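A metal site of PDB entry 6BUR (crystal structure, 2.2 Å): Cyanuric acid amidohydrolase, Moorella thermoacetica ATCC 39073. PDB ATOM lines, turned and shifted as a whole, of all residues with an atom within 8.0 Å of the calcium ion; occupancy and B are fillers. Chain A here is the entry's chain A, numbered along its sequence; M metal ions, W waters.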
ATOM      1  N   TRP A 222     -14.871 -34.951  20.016  1.00  0.00           N
ATOM      2  CA  TRP A 222     -13.733 -34.218  19.475  1.00  0.00           C
ATOM      3  C   TRP A 222     -13.023 -34.951  18.346  1.00  0.00           C
ATOM      4  O   TRP A 222     -12.180 -34.349  17.681  1.00  0.00           O
ATOM      5  CB  TRP A 222     -12.725 -33.895  20.587  1.00  0.00           C
ATOM      6  CG  TRP A 222     -13.316 -33.121  21.729  1.00  0.00           C
ATOM      7  CD1 TRP A 222     -13.294 -33.462  23.062  1.00  0.00           C
ATOM      8  CD2 TRP A 222     -14.038 -31.879  21.644  1.00  0.00           C
ATOM      9  NE1 TRP A 222     -13.967 -32.508  23.804  1.00  0.00           N
ATOM     10  CE2 TRP A 222     -14.424 -31.529  22.961  1.00  0.00           C
ATOM     11  CE3 TRP A 222     -14.408 -31.030  20.595  1.00  0.00           C
ATOM     12  CZ2 TRP A 222     -15.161 -30.363  23.249  1.00  0.00           C
ATOM     13  CZ3 TRP A 222     -15.130 -29.870  20.888  1.00  0.00           C
ATOM     14  CH2 TRP A 222     -15.494 -29.546  22.205  1.00  0.00           C
ATOM     15  N   LEU A 224     -14.578 -35.825  15.701  1.00  0.00           N
ATOM     16  CA  LEU A 224     -15.134 -35.177  14.526  1.00  0.00           C
ATOM     17  C   LEU A 224     -14.495 -33.806  14.389  1.00  0.00           C
ATOM     18  O   LEU A 224     -14.637 -32.962  15.290  1.00  0.00           O
ATOM     19  CB  LEU A 224     -16.652 -35.048  14.627  1.00  0.00           C
ATOM     20  CG  LEU A 224     -17.401 -36.344  14.863  1.00  0.00           C
ATOM     21  CD1 LEU A 224     -18.884 -36.069  15.009  1.00  0.00           C
ATOM     22  CD2 LEU A 224     -17.112 -37.297  13.720  1.00  0.00           C
ATOM     23  N   TYR A 225     -13.797 -33.566  13.276  1.00  0.00           N
ATOM     24  CA  TYR A 225     -13.303 -32.201  13.086  1.00  0.00           C
ATOM     25  C   TYR A 225     -12.986 -31.962  11.623  1.00  0.00           C
ATOM     26  O   TYR A 225     -12.766 -32.898  10.841  1.00  0.00           O
ATOM     27  CB  TYR A 225     -12.067 -31.920  13.943  1.00  0.00           C
ATOM     28  CG  TYR A 225     -10.870 -32.863  13.753  1.00  0.00           C
ATOM     29  CD1 TYR A 225      -9.904 -32.603  12.773  1.00  0.00           C
ATOM     30  CD2 TYR A 225     -10.717 -33.987  14.547  1.00  0.00           C
ATOM     31  CE1 TYR A 225      -8.800 -33.460  12.583  1.00  0.00           C
ATOM     32  CE2 TYR A 225      -9.616 -34.859  14.366  1.00  0.00           C
ATOM     33  CZ  TYR A 225      -8.660 -34.572  13.394  1.00  0.00           C
ATOM     34  OH  TYR A 225      -7.568 -35.379  13.248  1.00  0.00           O
ATOM     35  N   SER A 226     -12.959 -30.677  11.286  1.00  0.00           N
ATOM     36  CA  SER A 226     -12.473 -30.163  10.018  1.00  0.00           C
ATOM     37  C   SER A 226     -10.998 -29.797  10.139  1.00  0.00           C
ATOM     38  O   SER A 226     -10.534 -29.339  11.184  1.00  0.00           O
ATOM     39  CB  SER A 226     -13.273 -28.915   9.609  1.00  0.00           C
ATOM     40  OG  SER A 226     -12.811 -28.414   8.355  1.00  0.00           O
ATOM     41  N   ALA A 229     -11.249 -25.598   8.832  1.00  0.00           N
ATOM     42  CA  ALA A 229     -12.196 -24.653   9.433  1.00  0.00           C
ATOM     43  C   ALA A 229     -11.533 -23.796  10.505  1.00  0.00           C
ATOM     44  O   ALA A 229     -10.712 -24.282  11.297  1.00  0.00           O
ATOM     45  CB  ALA A 229     -13.384 -25.406  10.060  1.00  0.00           C
ATOM     46  N   VAL A 261      -2.083 -28.903   9.879  1.00  0.00           N
ATOM     47  CA  VAL A 261      -2.858 -28.931  11.114  1.00  0.00           C
ATOM     48  C   VAL A 261      -1.868 -29.055  12.264  1.00  0.00           C
ATOM     49  O   VAL A 261      -1.053 -29.989  12.276  1.00  0.00           O
ATOM     50  CB  VAL A 261      -3.872 -30.091  11.136  1.00  0.00           C
ATOM     51  CG1 VAL A 261      -4.626 -30.100  12.452  1.00  0.00           C
ATOM     52  CG2 VAL A 261      -4.842 -29.988   9.934  1.00  0.00           C
ATOM     53  N   MET A 262      -1.881 -28.097  13.166  1.00  0.00           N
ATOM     54  CA  MET A 262      -1.088 -28.224  14.375  1.00  0.00           C
ATOM     55  C   MET A 262      -1.687 -29.315  15.266  1.00  0.00           C
ATOM     56  O   MET A 262      -2.889 -29.289  15.571  1.00  0.00           O
ATOM     57  CB  MET A 262      -1.036 -26.896  15.149  1.00  0.00           C
ATOM     58  CG  MET A 262      -0.262 -25.764  14.466  1.00  0.00           C
ATOM     59  SD  MET A 262      -0.273 -24.232  15.451  1.00  0.00           S
ATOM     60  CE  MET A 262       1.094 -24.510  16.589  1.00  0.00           C
ATOM     61  N   LYS A 263      -0.845 -30.236  15.706  1.00  0.00           N
ATOM     62  CA  LYS A 263      -1.346 -31.321  16.546  1.00  0.00           C
ATOM     63  C   LYS A 263      -1.524 -30.872  17.986  1.00  0.00           C
ATOM     64  O   LYS A 263      -2.423 -31.382  18.682  1.00  0.00           O
ATOM     65  CB  LYS A 263      -0.410 -32.525  16.467  1.00  0.00           C
ATOM     66  CG  LYS A 263      -1.142 -33.837  16.504  1.00  0.00           C
ATOM     67  CD  LYS A 263      -2.191 -33.943  15.387  1.00  0.00           C
ATOM     68  CE  LYS A 263      -2.845 -35.323  15.338  1.00  0.00           C
ATOM     69  NZ  LYS A 263      -3.681 -35.639  16.533  1.00  0.00           N
ATOM     70  N   LYS A 295      -5.629 -21.533  14.229  1.00  0.00           N
ATOM     71  CA  LYS A 295      -6.471 -21.745  15.401  1.00  0.00           C
ATOM     72  C   LYS A 295      -5.632 -22.290  16.548  1.00  0.00           C
ATOM     73  O   LYS A 295      -4.680 -23.035  16.349  1.00  0.00           O
ATOM     74  CB  LYS A 295      -7.627 -22.709  15.085  1.00  0.00           C
ATOM     75  CG  LYS A 295      -8.753 -22.167  14.193  1.00  0.00           C
ATOM     76  CD  LYS A 295      -9.457 -20.926  14.812  1.00  0.00           C
ATOM     77  CE  LYS A 295     -10.053 -21.242  16.178  1.00  0.00           C
ATOM     78  NZ  LYS A 295     -11.074 -20.298  16.600  1.00  0.00           N
ATOM     79  N   ALA A 296      -6.016 -21.914  17.774  1.00  0.00           N
ATOM     80  CA  ALA A 296      -5.314 -22.311  18.998  1.00  0.00           C
ATOM     81  C   ALA A 296      -6.337 -22.772  20.025  1.00  0.00           C
ATOM     82  O   ALA A 296      -7.466 -22.275  20.047  1.00  0.00           O
ATOM     83  CB  ALA A 296      -4.473 -21.129  19.572  1.00  0.00           C
ATOM     84  N   GLU A 297      -5.942 -23.694  20.897  1.00  0.00           N
ATOM     85  CA  GLU A 297      -6.891 -24.056  21.950  1.00  0.00           C
ATOM     86  C   GLU A 297      -6.210 -24.810  23.079  1.00  0.00           C
ATOM     87  O   GLU A 297      -5.174 -25.454  22.902  1.00  0.00           O
ATOM     88  CB  GLU A 297      -8.056 -24.878  21.385  1.00  0.00           C
ATOM     89  CG  GLU A 297      -7.718 -26.310  21.036  1.00  0.00           C
ATOM     90  CD  GLU A 297      -8.956 -27.096  20.563  1.00  0.00           C
ATOM     91  OE1 GLU A 297     -10.106 -26.659  20.814  1.00  0.00           O
ATOM     92  OE2 GLU A 297      -8.755 -28.167  19.924  1.00  0.00           O
ATOM     93  N   ALA A 298      -6.819 -24.707  24.264  1.00  0.00           N
ATOM     94  CA  ALA A 298      -6.472 -25.564  25.393  1.00  0.00           C
ATOM     95  C   ALA A 298      -7.004 -26.967  25.154  1.00  0.00           C
ATOM     96  O   ALA A 298      -8.170 -27.134  24.814  1.00  0.00           O
ATOM     97  CB  ALA A 298      -7.086 -24.977  26.659  1.00  0.00           C
ATOM     98  N   ALA A 299      -6.162 -27.995  25.344  1.00  0.00           N
ATOM     99  CA  ALA A 299      -6.645 -29.359  25.149  1.00  0.00           C
ATOM    100  C   ALA A 299      -7.543 -29.778  26.315  1.00  0.00           C
ATOM    101  O   ALA A 299      -7.286 -29.428  27.469  1.00  0.00           O
ATOM    102  CB  ALA A 299      -5.480 -30.351  25.014  1.00  0.00           C
ATOM    103  N   GLY A 345     -10.011 -21.201  20.646  1.00  0.00           N
ATOM    104  CA  GLY A 345     -11.192 -22.037  20.708  1.00  0.00           C
ATOM    105  C   GLY A 345     -11.322 -22.821  19.423  1.00  0.00           C
ATOM    106  O   GLY A 345     -11.871 -22.322  18.434  1.00  0.00           O
ATOM    107  N   ALA A 346     -10.824 -24.065  19.406  1.00  0.00           N
ATOM    108  CA  ALA A 346     -10.724 -24.818  18.162  1.00  0.00           C
ATOM    109  C   ALA A 346     -11.600 -26.060  18.192  1.00  0.00           C
ATOM    110  O   ALA A 346     -11.186 -27.154  17.802  1.00  0.00           O
ATOM    111  CB  ALA A 346      -9.264 -25.176  17.851  1.00  0.00           C
ATOM    112  N   GLU A 347     -12.847 -25.882  18.642  1.00  0.00           N
ATOM    113  CA  GLU A 347     -13.808 -26.974  18.732  1.00  0.00           C
ATOM    114  C   GLU A 347     -14.090 -27.521  17.342  1.00  0.00           C
ATOM    115  O   GLU A 347     -14.523 -26.774  16.453  1.00  0.00           O
ATOM    116  CB  GLU A 347     -15.108 -26.496  19.384  1.00  0.00           C
ATOM    117  CG  GLU A 347     -14.958 -26.019  20.845  1.00  0.00           C
ATOM    118  CD  GLU A 347     -14.404 -24.591  20.986  1.00  0.00           C
ATOM    119  OE1 GLU A 347     -14.260 -23.879  19.970  1.00  0.00           O
ATOM    120  OE2 GLU A 347     -14.140 -24.183  22.137  1.00  0.00           O
ATOM    121  N   HIS A 348     -13.842 -28.820  17.148  1.00  0.00           N
ATOM    122  CA  HIS A 348     -14.074 -29.453  15.855  1.00  0.00           C
ATOM    123  C   HIS A 348     -13.247 -28.790  14.751  1.00  0.00           C
ATOM    124  O   HIS A 348     -13.622 -28.805  13.583  1.00  0.00           O
ATOM    125  CB  HIS A 348     -15.551 -29.432  15.492  1.00  0.00           C
ATOM    126  CG  HIS A 348     -16.429 -30.078  16.509  1.00  0.00           C
ATOM    127  ND1 HIS A 348     -16.367 -31.437  16.795  1.00  0.00           N
ATOM    128  CD2 HIS A 348     -17.403 -29.574  17.310  1.00  0.00           C
ATOM    129  CE1 HIS A 348     -17.252 -31.730  17.724  1.00  0.00           C
ATOM    130  NE2 HIS A 348     -17.898 -30.620  18.060  1.00  0.00           N
ATOM    131  N   GLN A 349     -12.127 -28.190  15.135  1.00  0.00           N
ATOM    132  CA  GLN A 349     -11.188 -27.566  14.202  1.00  0.00           C
ATOM    133  C   GLN A 349      -9.825 -28.152  14.538  1.00  0.00           C
ATOM    134  O   GLN A 349      -9.194 -27.748  15.525  1.00  0.00           O
ATOM    135  CB  GLN A 349     -11.183 -26.041  14.324  1.00  0.00           C
ATOM    136  CG  GLN A 349     -12.577 -25.399  14.101  1.00  0.00           C
ATOM    137  CD  GLN A 349     -12.711 -24.124  14.891  1.00  0.00           C
ATOM    138  OE1 GLN A 349     -12.112 -23.105  14.538  1.00  0.00           O
ATOM    139  NE2 GLN A 349     -13.446 -24.172  16.015  1.00  0.00           N
ATOM    140  N   GLY A 350      -9.376 -29.131  13.744  1.00  0.00           N
ATOM    141  CA  GLY A 350      -8.230 -29.918  14.114  1.00  0.00           C
ATOM    142  C   GLY A 350      -8.563 -30.788  15.320  1.00  0.00           C
ATOM    143  O   GLY A 350      -9.623 -30.641  15.940  1.00  0.00           O
ATOM    144  N   PRO A 351      -7.665 -31.714  15.657  1.00  0.00           N
ATOM    145  CA  PRO A 351      -7.892 -32.558  16.835  1.00  0.00           C
ATOM    146  C   PRO A 351      -7.972 -31.730  18.117  1.00  0.00           C
ATOM    147  O   PRO A 351      -7.679 -30.542  18.170  1.00  0.00           O
ATOM    148  CB  PRO A 351      -6.670 -33.481  16.842  1.00  0.00           C
ATOM    149  CG  PRO A 351      -5.605 -32.623  16.269  1.00  0.00           C
ATOM    150  CD  PRO A 351      -6.288 -31.831  15.157  1.00  0.00           C
ATOM    151  N   ASP A 352      -8.390 -32.412  19.168  1.00  0.00           N
ATOM    152  CA  ASP A 352      -8.510 -31.846  20.503  1.00  0.00           C
ATOM    153  C   ASP A 352      -7.149 -31.313  20.982  1.00  0.00           C
ATOM    154  O   ASP A 352      -6.207 -32.084  21.173  1.00  0.00           O
ATOM    155  CB  ASP A 352      -9.097 -32.927  21.413  1.00  0.00           C
ATOM    156  CG  ASP A 352      -9.214 -32.489  22.853  1.00  0.00           C
ATOM    157  OD1 ASP A 352      -8.962 -31.314  23.139  1.00  0.00           O
ATOM    158  OD2 ASP A 352      -9.558 -33.341  23.706  1.00  0.00           O
ATOM    159  N   GLY A 353      -7.025 -30.003  21.160  1.00  0.00           N
ATOM    160  CA  GLY A 353      -5.761 -29.386  21.524  1.00  0.00           C
ATOM    161  C   GLY A 353      -4.947 -28.824  20.365  1.00  0.00           C
ATOM    162  O   GLY A 353      -3.948 -28.144  20.618  1.00  0.00           O
ATOM    163  N   GLY A 354      -5.347 -29.094  19.130  1.00  0.00           N
ATOM    164  CA  GLY A 354      -4.688 -28.512  17.968  1.00  0.00           C
ATOM    165  C   GLY A 354      -5.665 -27.748  17.078  1.00  0.00           C
ATOM    166  O   GLY A 354      -6.845 -27.626  17.424  1.00  0.00           O
ATOM    167  N   GLY A 355      -5.196 -27.255  15.938  1.00  0.00           N
ATOM    168  CA  GLY A 355      -6.053 -26.594  14.984  1.00  0.00           C
ATOM    169  C   GLY A 355      -5.379 -26.312  13.652  1.00  0.00           C
ATOM    170  O   GLY A 355      -4.156 -26.338  13.531  1.00  0.00           O
ATOM    171  N   PRO A 356      -6.190 -26.022  12.624  1.00  0.00           N
ATOM    172  CA  PRO A 356      -5.623 -25.718  11.307  1.00  0.00           C
ATOM    173  C   PRO A 356      -4.699 -24.498  11.344  1.00  0.00           C
ATOM    174  O   PRO A 356      -4.853 -23.576  12.145  1.00  0.00           O
ATOM    175  CB  PRO A 356      -6.864 -25.427  10.451  1.00  0.00           C
ATOM    176  CG  PRO A 356      -7.991 -26.087  11.181  1.00  0.00           C
ATOM    177  CD  PRO A 356      -7.657 -25.934  12.628  1.00  0.00           C
HETATM  178 CA    CA M   1      -9.132 -28.636  17.729  1.00  0.00          CA
HETATM  179  O   HOH W   1     -10.992 -30.020  19.080  1.00  0.00           O
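The nearest printed residue that does not touch the calcium ion is Asp 352 (4.1 Å).
OE2 of Glu 297 binds the calcium ion, 2.3 Å away.
The backbone carbonyl oxygen (O) of Gln 349 is bound to the calcium ion (2.4 Å).
The calcium ion is bound by O of Pro 351, at 2.4 Å.
The backbone carbonyl oxygen (O) of Gly 354 is bound to the calcium ion (2.5 Å).
O of Ala 346 binds the calcium ion.
The calcium ion is bound by water W1 (2.7 Å).
O of Gly 350 is bound to the calcium ion, at 2.7 Å.
The side-chain carboxylate (OE2) of Glu 297 sits close to the backbone NH (N) of Gly 353 (2.8 Å).
N of Gly 350 is in hydrogen-bond range of O of Ser 226, 2.8 Å away.
The side-chain amide nitrogen of Gln 349 lies within hydrogen-bond range of the backbone carbonyl oxygen of Gly 345, 3.4 Å away.
NE2 of Gln 349 is in hydrogen-bond range of O of Glu 347 (2.8 Å).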
